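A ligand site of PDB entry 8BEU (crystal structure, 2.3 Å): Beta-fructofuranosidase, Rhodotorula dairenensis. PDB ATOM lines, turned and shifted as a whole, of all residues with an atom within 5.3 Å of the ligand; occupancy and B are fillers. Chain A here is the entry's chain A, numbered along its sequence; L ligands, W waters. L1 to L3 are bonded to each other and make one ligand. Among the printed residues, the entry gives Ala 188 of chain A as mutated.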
ATOM      1  N   ASN A 187     -18.356 -13.255 -19.436  1.00  0.00           N
ATOM      2  CA  ASN A 187     -17.001 -13.859 -19.321  1.00  0.00           C
ATOM      3  C   ASN A 187     -16.094 -13.155 -20.328  1.00  0.00           C
ATOM      4  O   ASN A 187     -16.044 -11.910 -20.290  1.00  0.00           O
ATOM      5  CB  ASN A 187     -17.041 -15.393 -19.293  1.00  0.00           C
ATOM      6  CG  ASN A 187     -17.753 -16.047 -20.442  1.00  0.00           C
ATOM      7  OD1 ASN A 187     -18.966 -16.032 -20.528  1.00  0.00           O
ATOM      8  ND2 ASN A 187     -17.000 -16.708 -21.289  1.00  0.00           N
ATOM      9  N   ALA A 188     -15.384 -13.903 -21.166  1.00  0.00           N
ATOM     10  CA  ALA A 188     -14.162 -13.472 -21.882  1.00  0.00           C
ATOM     11  C   ALA A 188     -14.400 -12.170 -22.651  1.00  0.00           C
ATOM     12  O   ALA A 188     -15.459 -11.970 -23.235  1.00  0.00           O
ATOM     13  CB  ALA A 188     -13.731 -14.583 -22.812  1.00  0.00           C
ATOM     14  N   GLN A 205     -18.370 -12.001 -24.039  1.00  0.00           N
ATOM     15  CA  GLN A 205     -19.267 -13.162 -23.905  1.00  0.00           C
ATOM     16  C   GLN A 205     -20.316 -12.790 -22.877  1.00  0.00           C
ATOM     17  O   GLN A 205     -19.931 -12.456 -21.752  1.00  0.00           O
ATOM     18  CB  GLN A 205     -18.465 -14.387 -23.482  1.00  0.00           C
ATOM     19  CG  GLN A 205     -17.544 -14.888 -24.595  1.00  0.00           C
ATOM     20  CD  GLN A 205     -18.403 -15.462 -25.703  1.00  0.00           C
ATOM     21  OE1 GLN A 205     -18.964 -16.547 -25.593  1.00  0.00           O
ATOM     22  NE2 GLN A 205     -18.526 -14.700 -26.766  1.00  0.00           N
ATOM     23  N   ALA A 213     -23.259 -19.083 -17.079  1.00  0.00           N
ATOM     24  CA  ALA A 213     -22.836 -19.116 -18.501  1.00  0.00           C
ATOM     25  C   ALA A 213     -23.956 -19.735 -19.363  1.00  0.00           C
ATOM     26  O   ALA A 213     -24.693 -20.600 -18.833  1.00  0.00           O
ATOM     27  CB  ALA A 213     -21.548 -19.880 -18.653  1.00  0.00           C
ATOM     28  N   GLY A 214     -24.048 -19.321 -20.619  1.00  0.00           N
ATOM     29  CA  GLY A 214     -25.004 -19.858 -21.613  1.00  0.00           C
ATOM     30  C   GLY A 214     -25.531 -18.767 -22.534  1.00  0.00           C
ATOM     31  O   GLY A 214     -25.202 -17.589 -22.299  1.00  0.00           O
ATOM     32  N   GLN A 216     -24.866 -17.501 -25.344  1.00  0.00           N
ATOM     33  CA  GLN A 216     -23.775 -16.500 -25.523  1.00  0.00           C
ATOM     34  C   GLN A 216     -24.107 -15.540 -26.673  1.00  0.00           C
ATOM     35  O   GLN A 216     -24.342 -16.013 -27.812  1.00  0.00           O
ATOM     36  CB  GLN A 216     -22.411 -17.162 -25.692  1.00  0.00           C
ATOM     37  CG  GLN A 216     -21.811 -17.665 -24.384  1.00  0.00           C
ATOM     38  CD  GLN A 216     -22.224 -19.075 -24.050  1.00  0.00           C
ATOM     39  OE1 GLN A 216     -23.201 -19.604 -24.567  1.00  0.00           O
ATOM     40  NE2 GLN A 216     -21.465 -19.709 -23.174  1.00  0.00           N
ATOM     41  N   PHE A 246     -19.625 -17.692 -29.541  1.00  0.00           N
ATOM     42  CA  PHE A 246     -18.438 -17.914 -28.697  1.00  0.00           C
ATOM     43  C   PHE A 246     -17.407 -16.832 -29.026  1.00  0.00           C
ATOM     44  O   PHE A 246     -17.732 -15.853 -29.745  1.00  0.00           O
ATOM     45  CB  PHE A 246     -17.994 -19.366 -28.889  1.00  0.00           C
ATOM     46  CG  PHE A 246     -18.729 -20.377 -28.035  1.00  0.00           C
ATOM     47  CD1 PHE A 246     -19.960 -20.089 -27.477  1.00  0.00           C
ATOM     48  CD2 PHE A 246     -18.152 -21.609 -27.751  1.00  0.00           C
ATOM     49  CE1 PHE A 246     -20.603 -21.013 -26.657  1.00  0.00           C
ATOM     50  CE2 PHE A 246     -18.807 -22.532 -26.958  1.00  0.00           C
ATOM     51  CZ  PHE A 246     -20.036 -22.230 -26.400  1.00  0.00           C
ATOM     52  N   SER A 247     -16.195 -16.949 -28.488  1.00  0.00           N
ATOM     53  CA  SER A 247     -15.200 -15.855 -28.509  1.00  0.00           C
ATOM     54  C   SER A 247     -14.719 -15.582 -29.945  1.00  0.00           C
ATOM     55  O   SER A 247     -14.959 -16.399 -30.834  1.00  0.00           O
ATOM     56  CB  SER A 247     -14.057 -16.143 -27.593  1.00  0.00           C
ATOM     57  OG  SER A 247     -14.515 -16.161 -26.254  1.00  0.00           O
ATOM     58  N   ASN A 275     -21.073 -21.775 -31.939  1.00  0.00           N
ATOM     59  CA  ASN A 275     -21.233 -23.091 -31.289  1.00  0.00           C
ATOM     60  C   ASN A 275     -22.617 -23.634 -31.640  1.00  0.00           C
ATOM     61  O   ASN A 275     -23.607 -22.897 -31.391  1.00  0.00           O
ATOM     62  CB  ASN A 275     -21.081 -23.007 -29.767  1.00  0.00           C
ATOM     63  CG  ASN A 275     -21.098 -24.375 -29.128  1.00  0.00           C
ATOM     64  OD1 ASN A 275     -20.266 -25.237 -29.460  1.00  0.00           O
ATOM     65  ND2 ASN A 275     -22.048 -24.592 -28.231  1.00  0.00           N
ATOM     66  N   GLN A 280     -18.198 -26.610 -33.751  1.00  0.00           N
ATOM     67  CA  GLN A 280     -17.671 -25.241 -33.576  1.00  0.00           C
ATOM     68  C   GLN A 280     -17.028 -24.830 -34.902  1.00  0.00           C
ATOM     69  O   GLN A 280     -16.107 -25.527 -35.344  1.00  0.00           O
ATOM     70  CB  GLN A 280     -16.703 -25.222 -32.393  1.00  0.00           C
ATOM     71  CG  GLN A 280     -17.422 -25.414 -31.052  1.00  0.00           C
ATOM     72  CD  GLN A 280     -16.537 -25.360 -29.841  1.00  0.00           C
ATOM     73  OE1 GLN A 280     -15.300 -25.336 -29.912  1.00  0.00           O
ATOM     74  NE2 GLN A 280     -17.195 -25.324 -28.706  1.00  0.00           N
ATOM     75  N   ASN A 308     -15.993 -30.262 -32.756  1.00  0.00           N
ATOM     76  CA  ASN A 308     -16.833 -29.494 -31.808  1.00  0.00           C
ATOM     77  C   ASN A 308     -15.943 -28.925 -30.674  1.00  0.00           C
ATOM     78  O   ASN A 308     -16.484 -28.564 -29.628  1.00  0.00           O
ATOM     79  CB  ASN A 308     -17.989 -30.435 -31.418  1.00  0.00           C
ATOM     80  CG  ASN A 308     -19.124 -29.769 -30.669  1.00  0.00           C
ATOM     81  OD1 ASN A 308     -19.468 -28.617 -30.930  1.00  0.00           O
ATOM     82  ND2 ASN A 308     -19.753 -30.517 -29.769  1.00  0.00           N
ATOM     83  N   GLN A 309     -14.628 -28.841 -30.920  1.00  0.00           N
ATOM     84  CA  GLN A 309     -13.612 -28.270 -30.001  1.00  0.00           C
ATOM     85  C   GLN A 309     -12.601 -27.497 -30.859  1.00  0.00           C
ATOM     86  O   GLN A 309     -11.466 -27.958 -31.001  1.00  0.00           O
ATOM     87  CB  GLN A 309     -12.956 -29.388 -29.182  1.00  0.00           C
ATOM     88  CG  GLN A 309     -13.933 -30.195 -28.342  1.00  0.00           C
ATOM     89  CD  GLN A 309     -14.628 -29.408 -27.263  1.00  0.00           C
ATOM     90  OE1 GLN A 309     -14.180 -28.329 -26.860  1.00  0.00           O
ATOM     91  NE2 GLN A 309     -15.740 -29.927 -26.784  1.00  0.00           N
ATOM     92  N   ARG A 311     -12.050 -23.271 -31.682  1.00  0.00           N
ATOM     93  CA  ARG A 311     -12.686 -21.982 -31.273  1.00  0.00           C
ATOM     94  C   ARG A 311     -11.644 -20.912 -30.915  1.00  0.00           C
ATOM     95  O   ARG A 311     -10.454 -21.239 -30.747  1.00  0.00           O
ATOM     96  CB  ARG A 311     -13.646 -22.206 -30.098  1.00  0.00           C
ATOM     97  CG  ARG A 311     -12.994 -22.795 -28.859  1.00  0.00           C
ATOM     98  CD  ARG A 311     -14.011 -22.895 -27.749  1.00  0.00           C
ATOM     99  NE  ARG A 311     -13.471 -23.481 -26.530  1.00  0.00           N
ATOM    100  CZ  ARG A 311     -13.279 -24.787 -26.338  1.00  0.00           C
ATOM    101  NH1 ARG A 311     -13.542 -25.643 -27.311  1.00  0.00           N
ATOM    102  NH2 ARG A 311     -12.802 -25.220 -25.183  1.00  0.00           N
ATOM    103  N   ASP A 312     -12.160 -19.676 -30.821  1.00  0.00           N
ATOM    104  CA  ASP A 312     -11.478 -18.456 -30.299  1.00  0.00           C
ATOM    105  C   ASP A 312     -10.459 -17.941 -31.317  1.00  0.00           C
ATOM    106  O   ASP A 312      -9.268 -17.819 -31.007  1.00  0.00           O
ATOM    107  CB  ASP A 312     -10.856 -18.726 -28.924  1.00  0.00           C
ATOM    108  CG  ASP A 312     -11.814 -19.358 -27.934  1.00  0.00           C
ATOM    109  OD1 ASP A 312     -13.040 -19.289 -28.167  1.00  0.00           O
ATOM    110  OD2 ASP A 312     -11.311 -19.937 -26.924  1.00  0.00           O
ATOM    111  N   GLU A 362      -7.094 -22.396 -25.111  1.00  0.00           N
ATOM    112  CA  GLU A 362      -8.216 -21.463 -25.387  1.00  0.00           C
ATOM    113  C   GLU A 362      -7.676 -20.059 -25.646  1.00  0.00           C
ATOM    114  O   GLU A 362      -6.516 -19.816 -25.332  1.00  0.00           O
ATOM    115  CB  GLU A 362      -9.196 -21.433 -24.214  1.00  0.00           C
ATOM    116  CG  GLU A 362      -9.927 -22.735 -24.010  1.00  0.00           C
ATOM    117  CD  GLU A 362     -10.996 -22.704 -22.930  1.00  0.00           C
ATOM    118  OE1 GLU A 362     -11.893 -23.584 -22.983  1.00  0.00           O
ATOM    119  OE2 GLU A 362     -10.953 -21.784 -22.038  1.00  0.00           O
ATOM    120  N   CYS A 363      -8.513 -19.213 -26.257  1.00  0.00           N
ATOM    121  CA  CYS A 363      -8.292 -17.751 -26.427  1.00  0.00           C
ATOM    122  C   CYS A 363      -6.830 -17.447 -26.794  1.00  0.00           C
ATOM    123  O   CYS A 363      -6.162 -16.633 -26.143  1.00  0.00           O
ATOM    124  CB  CYS A 363      -8.709 -17.031 -25.164  1.00  0.00           C
ATOM    125  SG  CYS A 363     -10.459 -17.304 -24.775  1.00  0.00           S
ATOM    126  N   ASN A 387      -7.997 -24.016 -19.403  1.00  0.00           N
ATOM    127  CA  ASN A 387      -9.102 -24.273 -18.459  1.00  0.00           C
ATOM    128  C   ASN A 387      -9.815 -25.568 -18.831  1.00  0.00           C
ATOM    129  O   ASN A 387     -10.020 -25.824 -20.018  1.00  0.00           O
ATOM    130  CB  ASN A 387     -10.140 -23.140 -18.455  1.00  0.00           C
ATOM    131  CG  ASN A 387     -11.280 -23.427 -17.502  1.00  0.00           C
ATOM    132  OD1 ASN A 387     -11.068 -23.581 -16.286  1.00  0.00           O
ATOM    133  ND2 ASN A 387     -12.483 -23.583 -18.031  1.00  0.00           N
ATOM    134  N   PRO A 388     -10.193 -26.428 -17.866  1.00  0.00           N
ATOM    135  CA  PRO A 388      -9.628 -26.410 -16.518  1.00  0.00           C
ATOM    136  C   PRO A 388      -8.151 -26.833 -16.508  1.00  0.00           C
ATOM    137  O   PRO A 388      -7.511 -26.766 -17.555  1.00  0.00           O
ATOM    138  CB  PRO A 388     -10.473 -27.438 -15.734  1.00  0.00           C
ATOM    139  CG  PRO A 388     -11.738 -27.583 -16.557  1.00  0.00           C
ATOM    140  CD  PRO A 388     -11.283 -27.406 -17.992  1.00  0.00           C
ATOM    141  N   TYR A 426      -7.935 -14.313 -16.597  1.00  0.00           N
ATOM    142  CA  TYR A 426      -8.158 -15.333 -17.632  1.00  0.00           C
ATOM    143  C   TYR A 426      -8.579 -14.665 -18.930  1.00  0.00           C
ATOM    144  O   TYR A 426      -9.264 -13.639 -18.876  1.00  0.00           O
ATOM    145  CB  TYR A 426      -9.240 -16.329 -17.220  1.00  0.00           C
ATOM    146  CG  TYR A 426      -9.291 -17.563 -18.087  1.00  0.00           C
ATOM    147  CD1 TYR A 426      -8.161 -18.373 -18.213  1.00  0.00           C
ATOM    148  CD2 TYR A 426     -10.439 -17.927 -18.780  1.00  0.00           C
ATOM    149  CE1 TYR A 426      -8.169 -19.500 -19.011  1.00  0.00           C
ATOM    150  CE2 TYR A 426     -10.458 -19.052 -19.591  1.00  0.00           C
ATOM    151  CZ  TYR A 426      -9.323 -19.842 -19.696  1.00  0.00           C
ATOM    152  OH  TYR A 426      -9.289 -20.969 -20.476  1.00  0.00           O
ATOM    153  N   ALA A 427      -8.208 -15.300 -20.053  1.00  0.00           N
ATOM    154  CA  ALA A 427      -8.759 -14.984 -21.390  1.00  0.00           C
ATOM    155  C   ALA A 427      -8.379 -13.561 -21.771  1.00  0.00           C
ATOM    156  O   ALA A 427      -9.204 -12.903 -22.372  1.00  0.00           O
ATOM    157  CB  ALA A 427     -10.255 -15.188 -21.394  1.00  0.00           C
ATOM    158  N   TRP A 448     -13.042 -19.990 -13.520  1.00  0.00           N
ATOM    159  CA  TRP A 448     -14.162 -20.904 -13.897  1.00  0.00           C
ATOM    160  C   TRP A 448     -14.609 -21.790 -12.736  1.00  0.00           C
ATOM    161  O   TRP A 448     -15.769 -22.234 -12.756  1.00  0.00           O
ATOM    162  CB  TRP A 448     -13.779 -21.719 -15.145  1.00  0.00           C
ATOM    163  CG  TRP A 448     -14.139 -20.954 -16.382  1.00  0.00           C
ATOM    164  CD1 TRP A 448     -13.281 -20.372 -17.259  1.00  0.00           C
ATOM    165  CD2 TRP A 448     -15.462 -20.583 -16.787  1.00  0.00           C
ATOM    166  NE1 TRP A 448     -13.991 -19.710 -18.217  1.00  0.00           N
ATOM    167  CE2 TRP A 448     -15.333 -19.840 -17.962  1.00  0.00           C
ATOM    168  CE3 TRP A 448     -16.750 -20.866 -16.312  1.00  0.00           C
ATOM    169  CZ2 TRP A 448     -16.441 -19.373 -18.680  1.00  0.00           C
ATOM    170  CZ3 TRP A 448     -17.846 -20.394 -17.010  1.00  0.00           C
ATOM    171  CH2 TRP A 448     -17.694 -19.640 -18.172  1.00  0.00           C
HETATM  172  C1  LIG L   1     -13.022 -19.223 -22.572  1.00  0.00           C
HETATM  173  C2  LIG L   1     -14.127 -19.816 -23.421  1.00  0.00           C
HETATM  174  C3  LIG L   1     -13.747 -19.770 -24.895  1.00  0.00           C
HETATM  175  C4  LIG L   1     -15.128 -19.718 -25.528  1.00  0.00           C
HETATM  176  C5  LIG L   1     -15.938 -18.912 -24.525  1.00  0.00           C
HETATM  177  C6  LIG L   1     -17.405 -19.301 -24.443  1.00  0.00           C
HETATM  178  O1  LIG L   1     -13.413 -19.338 -21.211  1.00  0.00           O
HETATM  179  O2  LIG L   1     -14.456 -21.140 -22.964  1.00  0.00           O
HETATM  180  O3  LIG L   1     -12.895 -20.865 -25.275  1.00  0.00           O
HETATM  181  O4  LIG L   1     -15.180 -19.095 -26.826  1.00  0.00           O
HETATM  182  O5  LIG L   1     -15.314 -19.054 -23.263  1.00  0.00           O
HETATM  183  O6  LIG L   1     -18.112 -18.317 -23.665  1.00  0.00           O
HETATM  184  C1  LG2 L   2     -15.360 -21.516 -21.923  1.00  0.00           C
HETATM  185  C2  LG2 L   2     -14.803 -22.561 -20.968  1.00  0.00           C
HETATM  186  C3  LG2 L   2     -14.768 -23.917 -21.652  1.00  0.00           C
HETATM  187  C4  LG2 L   2     -16.138 -24.211 -22.221  1.00  0.00           C
HETATM  188  C5  LG2 L   2     -16.625 -23.027 -23.073  1.00  0.00           C
HETATM  189  C6  LG2 L   2     -18.023 -23.259 -23.596  1.00  0.00           C
HETATM  190  O1  LG2 L   2     -13.460 -22.227 -20.588  1.00  0.00           O
HETATM  191  O2  LG2 L   2     -14.286 -24.958 -20.769  1.00  0.00           O
HETATM  192  O3  LG2 L   2     -15.974 -25.286 -23.123  1.00  0.00           O
HETATM  193  O4  LG2 L   2     -16.644 -21.795 -22.328  1.00  0.00           O
HETATM  194  O5  LG2 L   2     -18.821 -23.773 -22.488  1.00  0.00           O
HETATM  195  C1  LG3 L   3     -20.163 -23.871 -22.956  1.00  0.00           C
HETATM  196  C2  LG3 L   3     -20.996 -24.323 -21.760  1.00  0.00           C
HETATM  197  C3  LG3 L   3     -20.484 -25.739 -21.410  1.00  0.00           C
HETATM  198  C4  LG3 L   3     -20.484 -26.664 -22.645  1.00  0.00           C
HETATM  199  C5  LG3 L   3     -19.811 -26.001 -23.854  1.00  0.00           C
HETATM  200  C6  LG3 L   3     -19.970 -26.822 -25.125  1.00  0.00           C
HETATM  201  O1  LG3 L   3     -20.878 -23.416 -20.676  1.00  0.00           O
HETATM  202  O2  LG3 L   3     -21.264 -26.299 -20.360  1.00  0.00           O
HETATM  203  O3  LG3 L   3     -21.833 -26.984 -23.010  1.00  0.00           O
HETATM  204  O4  LG3 L   3     -20.345 -24.704 -24.112  1.00  0.00           O
HETATM  205  O5  LG3 L   3     -19.295 -26.195 -26.229  1.00  0.00           O
HETATM  206  O   HOH W   1     -16.642 -25.927 -25.708  1.00  0.00           O
HETATM  207  O   HOH W   2     -21.014 -27.858 -28.468  1.00  0.00           O
HETATM  208  O   HOH W   3     -22.890 -25.022 -25.104  1.00  0.00           O
HETATM  209  O   HOH W   4     -13.919 -17.099 -20.172  1.00  0.00           O
HETATM  210  O   HOH W   5     -18.522 -28.193 -28.384  1.00  0.00           O
HETATM  211  O   HOH W   6     -12.232 -26.014 -21.565  1.00  0.00           O
HETATM  212  O   HOH W   7     -19.513 -19.062 -21.473  1.00  0.00           O
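The backbone carbonyl oxygen of Gln 205 sits at hydrogen-bond distance from the backbone NH of Asn 187 (2.9 Å). The backbone carbonyl oxygen (O) of Phe 246 is in hydrogen-bond range of the side-chain amide nitrogen (NE2) of Gln 205 (3.3 Å). The side-chain hydroxyl (OH) of Tyr 426 sits at hydrogen-bond distance from the side-chain carboxylate (OE2) of Glu 362. The guanidinium group of Arg 311 sits at hydrogen-bond distance from the side-chain amide oxygen of Gln 280 (3.2 Å). The side-chain amide oxygen (OE1) of Gln 309 is in hydrogen-bond range of the guanidinium group (NH1) of Arg 311, at 2.8 Å. The backbone NH of Asn 387 lies close to the side-chain hydroxyl of Tyr 426, 3.5 Å away. The side-chain amide nitrogen (NE2) of Gln 280 sits at hydrogen-bond distance from the side-chain amide oxygen (OD1) of Asn 275, at 3.2 Å. NE2 of Gln 280 lies close to O of Asn 308 (3.4 Å).
Gln 216 touches the ligand. Phe 246 touches the ligand. OD1 of Asn 275 touches O5 of LG3 L3, 3.5 Å away. SG of Cys 363 touches C1 of LIG L1, 3.9 Å away. CE2 of Tyr 426 touches O1 of LIG L1 (3.4 Å). Hydrophobic or aromatic side chains within 4 Å of the ligand: Phe 246, Tyr 426 and Trp 448. Within 4 Å of the ligand: Asn 187, Gln 205, Gln 216, Phe 246, Ser 247, Asn 275, Gln 280, Arg 311, Asp 312, Glu 362, Cys 363, Asn 387, Tyr 426 and Trp 448. The nearest printed residue that does not touch the ligand is Ala 213 (4.1 Å).
The side-chain carboxylate of Asp 312 is in hydrogen-bond range of an oxygen (O3) of LIG L1 (2.5 Å). OE1 of Gln 205 is in hydrogen-bond range of O6 of LIG L1, 2.8 Å away. N of Ser 247 lies within hydrogen-bond range of O4 of LIG L1 (2.9 Å). The side-chain hydroxyl (OG) of Ser 247 sits at hydrogen-bond distance from an oxygen (O4) of LIG L1 (3.1 Å). The side-chain carboxylate (OE2) of Glu 362 sits at hydrogen-bond distance from an oxygen (O1) of LG2 L2, 2.9 Å away. NE of Arg 311 lies within hydrogen-bond range of O3 of LIG L1, 3.0 Å away. An oxygen (O1) of LG2 L2 lies within hydrogen-bond range of the side-chain amide nitrogen (ND2) of Asn 387 (3.1 Å). The indole nitrogen (NE1) of Trp 448 sits at hydrogen-bond distance from an oxygen (O1) of LIG L1 (3.1 Å). ND2 of Asn 187 sits at hydrogen-bond distance from O6 of LIG L1 (3.1 Å). The side-chain amide nitrogen of Gln 280 is in hydrogen-bond range of an oxygen (O5) of LG3 L3.
Water W6 lies within hydrogen-bond range of an oxygen (O2) of LG2 L2, the backbone carbonyl oxygen of Asn 387 and the side-chain carboxylate of Glu 362. Water W4 lies within hydrogen-bond range of O1 of LIG L1 (2.5 Å), NE1 of Trp 448 (3.3 Å) and ND2 of Asn 187 (3.3 Å). Water W7 lies within hydrogen-bond range of the side-chain amide nitrogen of Gln 216 (2.7 Å), an oxygen (O6) of LIG L1 (2.7 Å) and the side-chain amide oxygen of Asn 187 (3.2 Å). Water W1 bridges O5 of LG3 L3 (2.7 Å) and NE2 of Gln 280 (3.1 Å). Water W3 bridges an oxygen (O4) of LG3 L3 (2.7 Å) and the side-chain amide nitrogen (ND2) of Asn 275 (3.3 Å). Water W5 lies within hydrogen-bond range of O of Asn 308 (2.4 Å), O5 of LG3 L3 (3.0 Å) and NE2 of Gln 280 (3.2 Å).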
